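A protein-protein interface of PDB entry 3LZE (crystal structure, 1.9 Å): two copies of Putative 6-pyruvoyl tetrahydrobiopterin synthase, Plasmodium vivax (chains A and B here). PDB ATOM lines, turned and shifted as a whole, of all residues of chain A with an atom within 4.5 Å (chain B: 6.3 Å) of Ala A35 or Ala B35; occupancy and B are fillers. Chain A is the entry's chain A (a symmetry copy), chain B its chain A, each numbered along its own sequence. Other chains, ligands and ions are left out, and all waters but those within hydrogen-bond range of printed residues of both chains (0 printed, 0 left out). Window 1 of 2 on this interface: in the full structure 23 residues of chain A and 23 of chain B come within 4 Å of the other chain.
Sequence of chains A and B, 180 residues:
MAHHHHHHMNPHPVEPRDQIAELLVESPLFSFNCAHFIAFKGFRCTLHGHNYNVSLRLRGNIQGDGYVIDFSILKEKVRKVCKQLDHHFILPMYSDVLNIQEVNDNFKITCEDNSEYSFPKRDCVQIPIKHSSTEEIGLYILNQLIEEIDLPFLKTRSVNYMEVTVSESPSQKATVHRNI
The backbone NH of His B88 lies close to the backbone carbonyl oxygen of Leu A47, 3.5 Å away.
O of Leu B47 lies close to N of His A88, at 3.5 Å.
The backbone carbonyl oxygen (O) of Leu A47 lies close to the backbone carbonyl oxygen (O) of His B87 (3.4 Å).
Cys A34 touches His B48 (C to C, 3.9 Å).
Gly B49 touches Cys A34.
CB of Ala A35 touches CB of Ala B35, at 3.9 Å.
His A48 touches Asn B33 (CB to O, 3.2 Å).
Cys B34 touches His A48.
O of Gly A49 touches CB of Asn B33, 3.3 Å away.
Cys B34 touches Gly A49.
Ala B35 touches Gly A49.
Gly A49 touches His B50.
Phe A89 touches Leu B47 (N to O, 3.5 Å).
Of the 15 printed residues of chain B, 10 touch a printed residue of chain A.
Printed residues of chain B that touch a printed residue of chain A: Asn B33, Cys B34, Ala B35, Leu B47, His B48, Gly B49, His B50, His B87, His B88 and Phe B89.
Hydrophobic or aromatic side chains of chain B within 4 Å of the printed part of chain A: Ala B35 and His B87.
Printed residues of chain A that touch a printed residue of chain B: Cys A34, Ala A35, Leu A47, His A48, Gly A49, His A88 and Phe A89.
Hydrophobic or aromatic side chains of chain A within 4 Å of the printed part of chain B: Ala A35 and His A48.
Cys A34 touches Gly B49, and with the chains exchanged Gly A49 touches Cys B34.
Ala B35 touches its own counterpart, Ala A35.
Ala A35 touches His B48, and with the chains exchanged His A48 touches Ala B35.
Ala A35 touches Gly B49, and with the chains exchanged Gly A49 touches Ala B35.
Positions printed for both chains: 34, 35, 36, 47, 48, 49, 88, 89 and 90.
Of the 19 pairs that touch across the chains among the printed residues, 14 have their exchanged pair printed and touching as well.
Of the printed residues of chain B, Leu A47 touches His B87 (3.4 Å), His B88 (3.3 Å) and Phe B89 (3.5 Å).
Of the printed residues of chain B, Gly A49 touches Asn B33, Cys B34, Ala B35, Gly B49 and His B50.
Of the printed residues of chain B, His A88 touches Leu B47 (3.3 Å).
Ala B35 touches just these residues of chain A: Ala A35 (3.9 Å), His A48 (3.6 Å) and Gly A49 (3.8 Å).
Of the printed residues of chain A, Gly B49 touches Cys A34, Ala A35 and Gly A49.
Of the printed residues of chain A, His B88 touches Leu A47.
The nearest residue of chain B that does not touch Ala A35 is Leu B47 (4.1 Å).
The nearest residue of chain A that does not touch Ala B35 is Leu A47 (4.1 Å).
The nearest printed residue of chain A that does not touch Cys B34 is Cys A34 (5.4 Å).
O of Cys B34 is in hydrogen-bond range of N of His B50.
The backbone NH (N) of Ala B35 is in hydrogen-bond range of the backbone carbonyl oxygen (O) of His B88.
N of Ala A35 sits at hydrogen-bond distance from O of His A88, 3.1 Å away.
The backbone NH (N) of Ile B90 sits at hydrogen-bond distance from the backbone carbonyl oxygen (O) of Ala B35, 3.0 Å away.
The backbone carbonyl oxygen (O) of Asn B33 is in hydrogen-bond range of the backbone NH (N) of His B87 (2.9 Å).
N of Ile A90 sits at hydrogen-bond distance from O of Ala A35, 3.0 Å away.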
ATOM      1  N   CYS A  34      16.323   8.271 -23.723  1.00  0.00           N
ATOM      2  CA  CYS A  34      16.517   9.607 -23.230  1.00  0.00           C
ATOM      3  C   CYS A  34      15.625  10.612 -23.950  1.00  0.00           C
ATOM      4  O   CYS A  34      15.140  10.344 -25.054  1.00  0.00           O
ATOM      5  CB  CYS A  34      17.972  10.027 -23.446  1.00  0.00           C
ATOM      6  SG  CYS A  34      19.094   9.130 -22.310  1.00  0.00           S
ATOM      7  N   ALA A  35      15.386  11.745 -23.297  1.00  0.00           N
ATOM      8  CA  ALA A  35      14.728  12.890 -23.902  1.00  0.00           C
ATOM      9  C   ALA A  35      15.841  13.836 -24.302  1.00  0.00           C
ATOM     10  O   ALA A  35      16.880  13.858 -23.650  1.00  0.00           O
ATOM     11  CB  ALA A  35      13.766  13.592 -22.913  1.00  0.00           C
ATOM     12  N   HIS A  36      15.588  14.667 -25.305  1.00  0.00           N
ATOM     13  CA  HIS A  36      16.549  15.723 -25.681  1.00  0.00           C
ATOM     14  C   HIS A  36      15.804  16.687 -26.604  1.00  0.00           C
ATOM     15  O   HIS A  36      14.628  16.478 -26.912  1.00  0.00           O
ATOM     16  CB  HIS A  36      17.748  15.150 -26.368  1.00  0.00           C
ATOM     17  CG  HIS A  36      17.550  14.910 -27.836  1.00  0.00           C
ATOM     18  ND1 HIS A  36      18.412  15.422 -28.775  1.00  0.00           N
ATOM     19  CD2 HIS A  36      16.591  14.240 -28.526  1.00  0.00           C
ATOM     20  CE1 HIS A  36      18.000  15.067 -29.990  1.00  0.00           C
ATOM     21  NE2 HIS A  36      16.913  14.337 -29.859  1.00  0.00           N
ATOM     22  N   LEU A  47      10.923  19.293 -27.639  1.00  0.00           N
ATOM     23  CA  LEU A  47      11.251  18.190 -26.779  1.00  0.00           C
ATOM     24  C   LEU A  47      10.634  16.883 -27.251  1.00  0.00           C
ATOM     25  O   LEU A  47       9.435  16.796 -27.564  1.00  0.00           O
ATOM     26  CB  LEU A  47      10.734  18.465 -25.374  1.00  0.00           C
ATOM     27  CG  LEU A  47      11.043  17.428 -24.301  1.00  0.00           C
ATOM     28  CD1 LEU A  47      12.518  17.418 -24.022  1.00  0.00           C
ATOM     29  CD2 LEU A  47      10.222  17.793 -23.027  1.00  0.00           C
ATOM     30  N   HIS A  48      11.471  15.857 -27.251  1.00  0.00           N
ATOM     31  CA  HIS A  48      11.096  14.527 -27.694  1.00  0.00           C
ATOM     32  C   HIS A  48      12.109  13.573 -27.111  1.00  0.00           C
ATOM     33  O   HIS A  48      12.797  13.942 -26.159  1.00  0.00           O
ATOM     34  CB  HIS A  48      11.058  14.472 -29.224  1.00  0.00           C
ATOM     35  CG  HIS A  48      12.384  14.690 -29.913  1.00  0.00           C
ATOM     36  ND1 HIS A  48      12.859  15.950 -30.243  1.00  0.00           N
ATOM     37  CD2 HIS A  48      13.249  13.809 -30.463  1.00  0.00           C
ATOM     38  CE1 HIS A  48      14.009  15.825 -30.889  1.00  0.00           C
ATOM     39  NE2 HIS A  48      14.270  14.534 -31.034  1.00  0.00           N
ATOM     40  N   GLY A  49      12.269  12.394 -27.706  1.00  0.00           N
ATOM     41  CA  GLY A  49      13.091  11.378 -27.118  1.00  0.00           C
ATOM     42  C   GLY A  49      13.406  10.261 -28.075  1.00  0.00           C
ATOM     43  O   GLY A  49      12.873  10.205 -29.183  1.00  0.00           O
ATOM     44  N   HIS A  88      17.116   9.732 -18.705  1.00  0.00           N
ATOM     45  CA  HIS A  88      17.399  11.116 -18.361  1.00  0.00           C
ATOM     46  C   HIS A  88      17.176  12.005 -19.573  1.00  0.00           C
ATOM     47  O   HIS A  88      17.148  11.529 -20.715  1.00  0.00           O
ATOM     48  CB  HIS A  88      18.866  11.321 -17.924  1.00  0.00           C
ATOM     49  CG  HIS A  88      19.192  10.698 -16.612  1.00  0.00           C
ATOM     50  ND1 HIS A  88      19.639   9.404 -16.502  1.00  0.00           N
ATOM     51  CD2 HIS A  88      19.167  11.198 -15.354  1.00  0.00           C
ATOM     52  CE1 HIS A  88      19.856   9.122 -15.230  1.00  0.00           C
ATOM     53  NE2 HIS A  88      19.566  10.189 -14.513  1.00  0.00           N
ATOM     54  N   PHE A  89      17.019  13.290 -19.297  1.00  0.00           N
ATOM     55  CA  PHE A  89      17.156  14.327 -20.295  1.00  0.00           C
ATOM     56  C   PHE A  89      18.626  14.641 -20.480  1.00  0.00           C
ATOM     57  O   PHE A  89      19.366  14.917 -19.522  1.00  0.00           O
ATOM     58  CB  PHE A  89      16.356  15.587 -19.893  1.00  0.00           C
ATOM     59  CG  PHE A  89      16.536  16.727 -20.859  1.00  0.00           C
ATOM     60  CD1 PHE A  89      15.722  16.825 -21.991  1.00  0.00           C
ATOM     61  CD2 PHE A  89      17.479  17.713 -20.620  1.00  0.00           C
ATOM     62  CE1 PHE A  89      15.908  17.842 -22.923  1.00  0.00           C
ATOM     63  CE2 PHE A  89      17.622  18.770 -21.533  1.00  0.00           C
ATOM     64  CZ  PHE A  89      16.861  18.825 -22.669  1.00  0.00           C
ATOM     65  N   ILE A  90      19.055  14.646 -21.729  1.00  0.00           N
ATOM     66  CA  ILE A  90      20.444  14.876 -22.059  1.00  0.00           C
ATOM     67  C   ILE A  90      20.661  16.344 -22.207  1.00  0.00           C
ATOM     68  O   ILE A  90      20.106  16.981 -23.100  1.00  0.00           O
ATOM     69  CB  ILE A  90      20.848  14.156 -23.344  1.00  0.00           C
ATOM     70  CG1 ILE A  90      20.804  12.647 -23.124  1.00  0.00           C
ATOM     71  CG2 ILE A  90      22.282  14.597 -23.785  1.00  0.00           C
ATOM     72  CD1 ILE A  90      20.942  11.843 -24.453  1.00  0.00           C
ATOM     73  N   ASN B  33       8.709   9.676 -31.986  1.00  0.00           N
ATOM     74  CA  ASN B  33       9.831   9.804 -31.104  1.00  0.00           C
ATOM     75  C   ASN B  33       9.426  10.848 -30.048  1.00  0.00           C
ATOM     76  O   ASN B  33       9.339  12.041 -30.358  1.00  0.00           O
ATOM     77  CB  ASN B  33      11.062  10.198 -31.923  1.00  0.00           C
ATOM     78  CG  ASN B  33      11.394   9.156 -33.036  1.00  0.00           C
ATOM     79  OD1 ASN B  33      10.927   8.002 -33.021  1.00  0.00           O
ATOM     80  ND2 ASN B  33      12.173   9.578 -34.003  1.00  0.00           N
ATOM     81  N   CYS B  34       9.084  10.386 -28.841  1.00  0.00           N
ATOM     82  CA  CYS B  34       8.473  11.223 -27.846  1.00  0.00           C
ATOM     83  C   CYS B  34       9.191  11.127 -26.504  1.00  0.00           C
ATOM     84  O   CYS B  34       9.913  10.158 -26.247  1.00  0.00           O
ATOM     85  CB  CYS B  34       7.019  10.795 -27.636  1.00  0.00           C
ATOM     86  SG  CYS B  34       5.983  11.247 -29.075  1.00  0.00           S
ATOM     87  N   ALA B  35       9.015  12.153 -25.678  1.00  0.00           N
ATOM     88  CA  ALA B  35       9.455  12.147 -24.293  1.00  0.00           C
ATOM     89  C   ALA B  35       8.226  11.811 -23.476  1.00  0.00           C
ATOM     90  O   ALA B  35       7.118  12.147 -23.884  1.00  0.00           O
ATOM     91  CB  ALA B  35      10.019  13.523 -23.861  1.00  0.00           C
ATOM     92  N   HIS B  36       8.430  11.236 -22.298  1.00  0.00           N
ATOM     93  CA  HIS B  36       7.311  10.997 -21.363  1.00  0.00           C
ATOM     94  C   HIS B  36       7.936  10.665 -20.008  1.00  0.00           C
ATOM     95  O   HIS B  36       9.161  10.615 -19.877  1.00  0.00           O
ATOM     96  CB  HIS B  36       6.437   9.879 -21.834  1.00  0.00           C
ATOM     97  CG  HIS B  36       6.942   8.515 -21.464  1.00  0.00           C
ATOM     98  ND1 HIS B  36       6.156   7.610 -20.794  1.00  0.00           N
ATOM     99  CD2 HIS B  36       8.146   7.911 -21.645  1.00  0.00           C
ATOM    100  CE1 HIS B  36       6.850   6.494 -20.585  1.00  0.00           C
ATOM    101  NE2 HIS B  36       8.047   6.649 -21.110  1.00  0.00           N
ATOM    102  N   PHE B  37       7.109  10.480 -19.014  1.00  0.00           N
ATOM    103  CA  PHE B  37       7.595   9.901 -17.809  1.00  0.00           C
ATOM    104  C   PHE B  37       6.397   9.229 -17.185  1.00  0.00           C
ATOM    105  O   PHE B  37       5.294   9.675 -17.366  1.00  0.00           O
ATOM    106  CB  PHE B  37       8.298  10.921 -16.865  1.00  0.00           C
ATOM    107  CG  PHE B  37       7.379  12.004 -16.258  1.00  0.00           C
ATOM    108  CD1 PHE B  37       6.635  11.745 -15.111  1.00  0.00           C
ATOM    109  CD2 PHE B  37       7.448  13.321 -16.715  1.00  0.00           C
ATOM    110  CE1 PHE B  37       5.859  12.767 -14.495  1.00  0.00           C
ATOM    111  CE2 PHE B  37       6.696  14.336 -16.127  1.00  0.00           C
ATOM    112  CZ  PHE B  37       5.872  14.041 -15.008  1.00  0.00           C
ATOM    113  N   LEU B  47      12.095  11.824 -16.396  1.00  0.00           N
ATOM    114  CA  LEU B  47      11.914  12.159 -17.781  1.00  0.00           C
ATOM    115  C   LEU B  47      12.917  11.457 -18.684  1.00  0.00           C
ATOM    116  O   LEU B  47      14.133  11.449 -18.437  1.00  0.00           O
ATOM    117  CB  LEU B  47      12.091  13.659 -17.971  1.00  0.00           C
ATOM    118  CG  LEU B  47      11.874  14.215 -19.373  1.00  0.00           C
ATOM    119  CD1 LEU B  47      10.425  14.090 -19.745  1.00  0.00           C
ATOM    120  CD2 LEU B  47      12.340  15.703 -19.380  1.00  0.00           C
ATOM    121  N   HIS B  48      12.382  10.906 -19.763  1.00  0.00           N
ATOM    122  CA  HIS B  48      13.154  10.163 -20.740  1.00  0.00           C
ATOM    123  C   HIS B  48      12.332  10.121 -22.005  1.00  0.00           C
ATOM    124  O   HIS B  48      11.418  10.932 -22.147  1.00  0.00           O
ATOM    125  CB  HIS B  48      13.471   8.762 -20.206  1.00  0.00           C
ATOM    126  CG  HIS B  48      12.275   7.870 -19.979  1.00  0.00           C
ATOM    127  ND1 HIS B  48      11.559   7.863 -18.791  1.00  0.00           N
ATOM    128  CD2 HIS B  48      11.772   6.859 -20.723  1.00  0.00           C
ATOM    129  CE1 HIS B  48      10.610   6.942 -18.861  1.00  0.00           C
ATOM    130  NE2 HIS B  48      10.716   6.319 -20.025  1.00  0.00           N
ATOM    131  N   GLY B  49      12.584   9.151 -22.880  1.00  0.00           N
ATOM    132  CA  GLY B  49      11.958   9.142 -24.170  1.00  0.00           C
ATOM    133  C   GLY B  49      12.110   7.825 -24.878  1.00  0.00           C
ATOM    134  O   GLY B  49      12.824   6.935 -24.418  1.00  0.00           O
ATOM    135  N   HIS B  50      11.436   7.716 -26.008  1.00  0.00           N
ATOM    136  CA  HIS B  50      11.371   6.486 -26.787  1.00  0.00           C
ATOM    137  C   HIS B  50      11.043   6.759 -28.237  1.00  0.00           C
ATOM    138  O   HIS B  50      10.344   7.747 -28.557  1.00  0.00           O
ATOM    139  CB  HIS B  50      10.265   5.572 -26.303  1.00  0.00           C
ATOM    140  CG  HIS B  50      10.389   5.149 -24.883  1.00  0.00           C
ATOM    141  ND1 HIS B  50      11.385   4.304 -24.437  1.00  0.00           N
ATOM    142  CD2 HIS B  50       9.616   5.431 -23.808  1.00  0.00           C
ATOM    143  CE1 HIS B  50      11.231   4.099 -23.139  1.00  0.00           C
ATOM    144  NE2 HIS B  50      10.173   4.784 -22.733  1.00  0.00           N
ATOM    145  N   TYR B  52       8.735   5.211 -30.289  1.00  0.00           N
ATOM    146  CA  TYR B  52       7.609   4.299 -30.253  1.00  0.00           C
ATOM    147  C   TYR B  52       7.360   3.838 -31.659  1.00  0.00           C
ATOM    148  O   TYR B  52       7.534   4.604 -32.617  1.00  0.00           O
ATOM    149  CB  TYR B  52       6.366   5.003 -29.718  1.00  0.00           C
ATOM    150  CG  TYR B  52       6.396   5.367 -28.247  1.00  0.00           C
ATOM    151  CD1 TYR B  52       5.854   4.521 -27.293  1.00  0.00           C
ATOM    152  CD2 TYR B  52       6.892   6.601 -27.810  1.00  0.00           C
ATOM    153  CE1 TYR B  52       5.812   4.885 -25.956  1.00  0.00           C
ATOM    154  CE2 TYR B  52       6.838   6.964 -26.472  1.00  0.00           C
ATOM    155  CZ  TYR B  52       6.300   6.100 -25.546  1.00  0.00           C
ATOM    156  OH  TYR B  52       6.253   6.465 -24.197  1.00  0.00           O
ATOM    157  N   HIS B  87       7.726  13.819 -32.014  1.00  0.00           N
ATOM    158  CA  HIS B  87       8.485  14.993 -31.565  1.00  0.00           C
ATOM    159  C   HIS B  87       7.778  15.871 -30.501  1.00  0.00           C
ATOM    160  O   HIS B  87       7.803  17.094 -30.584  1.00  0.00           O
ATOM    161  CB  HIS B  87       8.963  15.802 -32.786  1.00  0.00           C
ATOM    162  CG  HIS B  87      10.272  15.318 -33.317  1.00  0.00           C
ATOM    163  ND1 HIS B  87      11.334  16.161 -33.562  1.00  0.00           N
ATOM    164  CD2 HIS B  87      10.717  14.065 -33.572  1.00  0.00           C
ATOM    165  CE1 HIS B  87      12.367  15.452 -33.987  1.00  0.00           C
ATOM    166  NE2 HIS B  87      12.018  14.176 -34.005  1.00  0.00           N
ATOM    167  N   HIS B  88       7.083  15.228 -29.544  1.00  0.00           N
ATOM    168  CA  HIS B  88       6.401  15.923 -28.465  1.00  0.00           C
ATOM    169  C   HIS B  88       6.597  15.170 -27.160  1.00  0.00           C
ATOM    170  O   HIS B  88       6.945  13.982 -27.157  1.00  0.00           O
ATOM    171  CB  HIS B  88       4.878  16.014 -28.699  1.00  0.00           C
ATOM    172  CG  HIS B  88       4.497  16.919 -29.818  1.00  0.00           C
ATOM    173  ND1 HIS B  88       4.382  16.480 -31.114  1.00  0.00           N
ATOM    174  CD2 HIS B  88       4.174  18.233 -29.834  1.00  0.00           C
ATOM    175  CE1 HIS B  88       4.026  17.489 -31.889  1.00  0.00           C
ATOM    176  NE2 HIS B  88       3.905  18.566 -31.139  1.00  0.00           N
ATOM    177  N   PHE B  89       6.372  15.883 -26.068  1.00  0.00           N
ATOM    178  CA  PHE B  89       6.151  15.282 -24.771  1.00  0.00           C
ATOM    179  C   PHE B  89       4.705  14.842 -24.672  1.00  0.00           C
ATOM    180  O   PHE B  89       3.764  15.615 -24.913  1.00  0.00           O
ATOM    181  CB  PHE B  89       6.521  16.265 -23.639  1.00  0.00           C
ATOM    182  CG  PHE B  89       6.228  15.716 -22.269  1.00  0.00           C
ATOM    183  CD1 PHE B  89       7.174  14.926 -21.610  1.00  0.00           C
ATOM    184  CD2 PHE B  89       5.038  16.017 -21.626  1.00  0.00           C
ATOM    185  CE1 PHE B  89       6.901  14.366 -20.366  1.00  0.00           C
ATOM    186  CE2 PHE B  89       4.792  15.498 -20.345  1.00  0.00           C
ATOM    187  CZ  PHE B  89       5.699  14.677 -19.734  1.00  0.00           C
ATOM    188  N   ILE B  90       4.513  13.599 -24.272  1.00  0.00           N
ATOM    189  CA  ILE B  90       3.191  13.021 -24.180  1.00  0.00           C
ATOM    190  C   ILE B  90       2.637  13.314 -22.827  1.00  0.00           C
ATOM    191  O   ILE B  90       3.159  12.852 -21.813  1.00  0.00           O
ATOM    192  CB  ILE B  90       3.215  11.512 -24.419  1.00  0.00           C
ATOM    193  CG1 ILE B  90       3.602  11.228 -25.867  1.00  0.00           C
ATOM    194  CG2 ILE B  90       1.814  10.891 -24.102  1.00  0.00           C
ATOM    195  CD1 ILE B  90       3.908   9.719 -26.121  1.00  0.00           C
ATOM    196  N   LEU B  91       1.532  14.065 -22.793  1.00  0.00           N
ATOM    197  CA  LEU B  91       0.976  14.518 -21.548  1.00  0.00           C
ATOM    198  C   LEU B  91      -0.399  13.933 -21.309  1.00  0.00           C
ATOM    199  O   LEU B  91      -1.364  14.257 -22.003  1.00  0.00           O
ATOM    200  CB  LEU B  91       0.915  16.036 -21.549  1.00  0.00           C
ATOM    201  CG  LEU B  91       0.558  16.819 -20.306  1.00  0.00           C
ATOM    202  CD1 LEU B  91       1.568  16.547 -19.212  1.00  0.00           C
ATOM    203  CD2 LEU B  91       0.513  18.286 -20.653  1.00  0.00           C
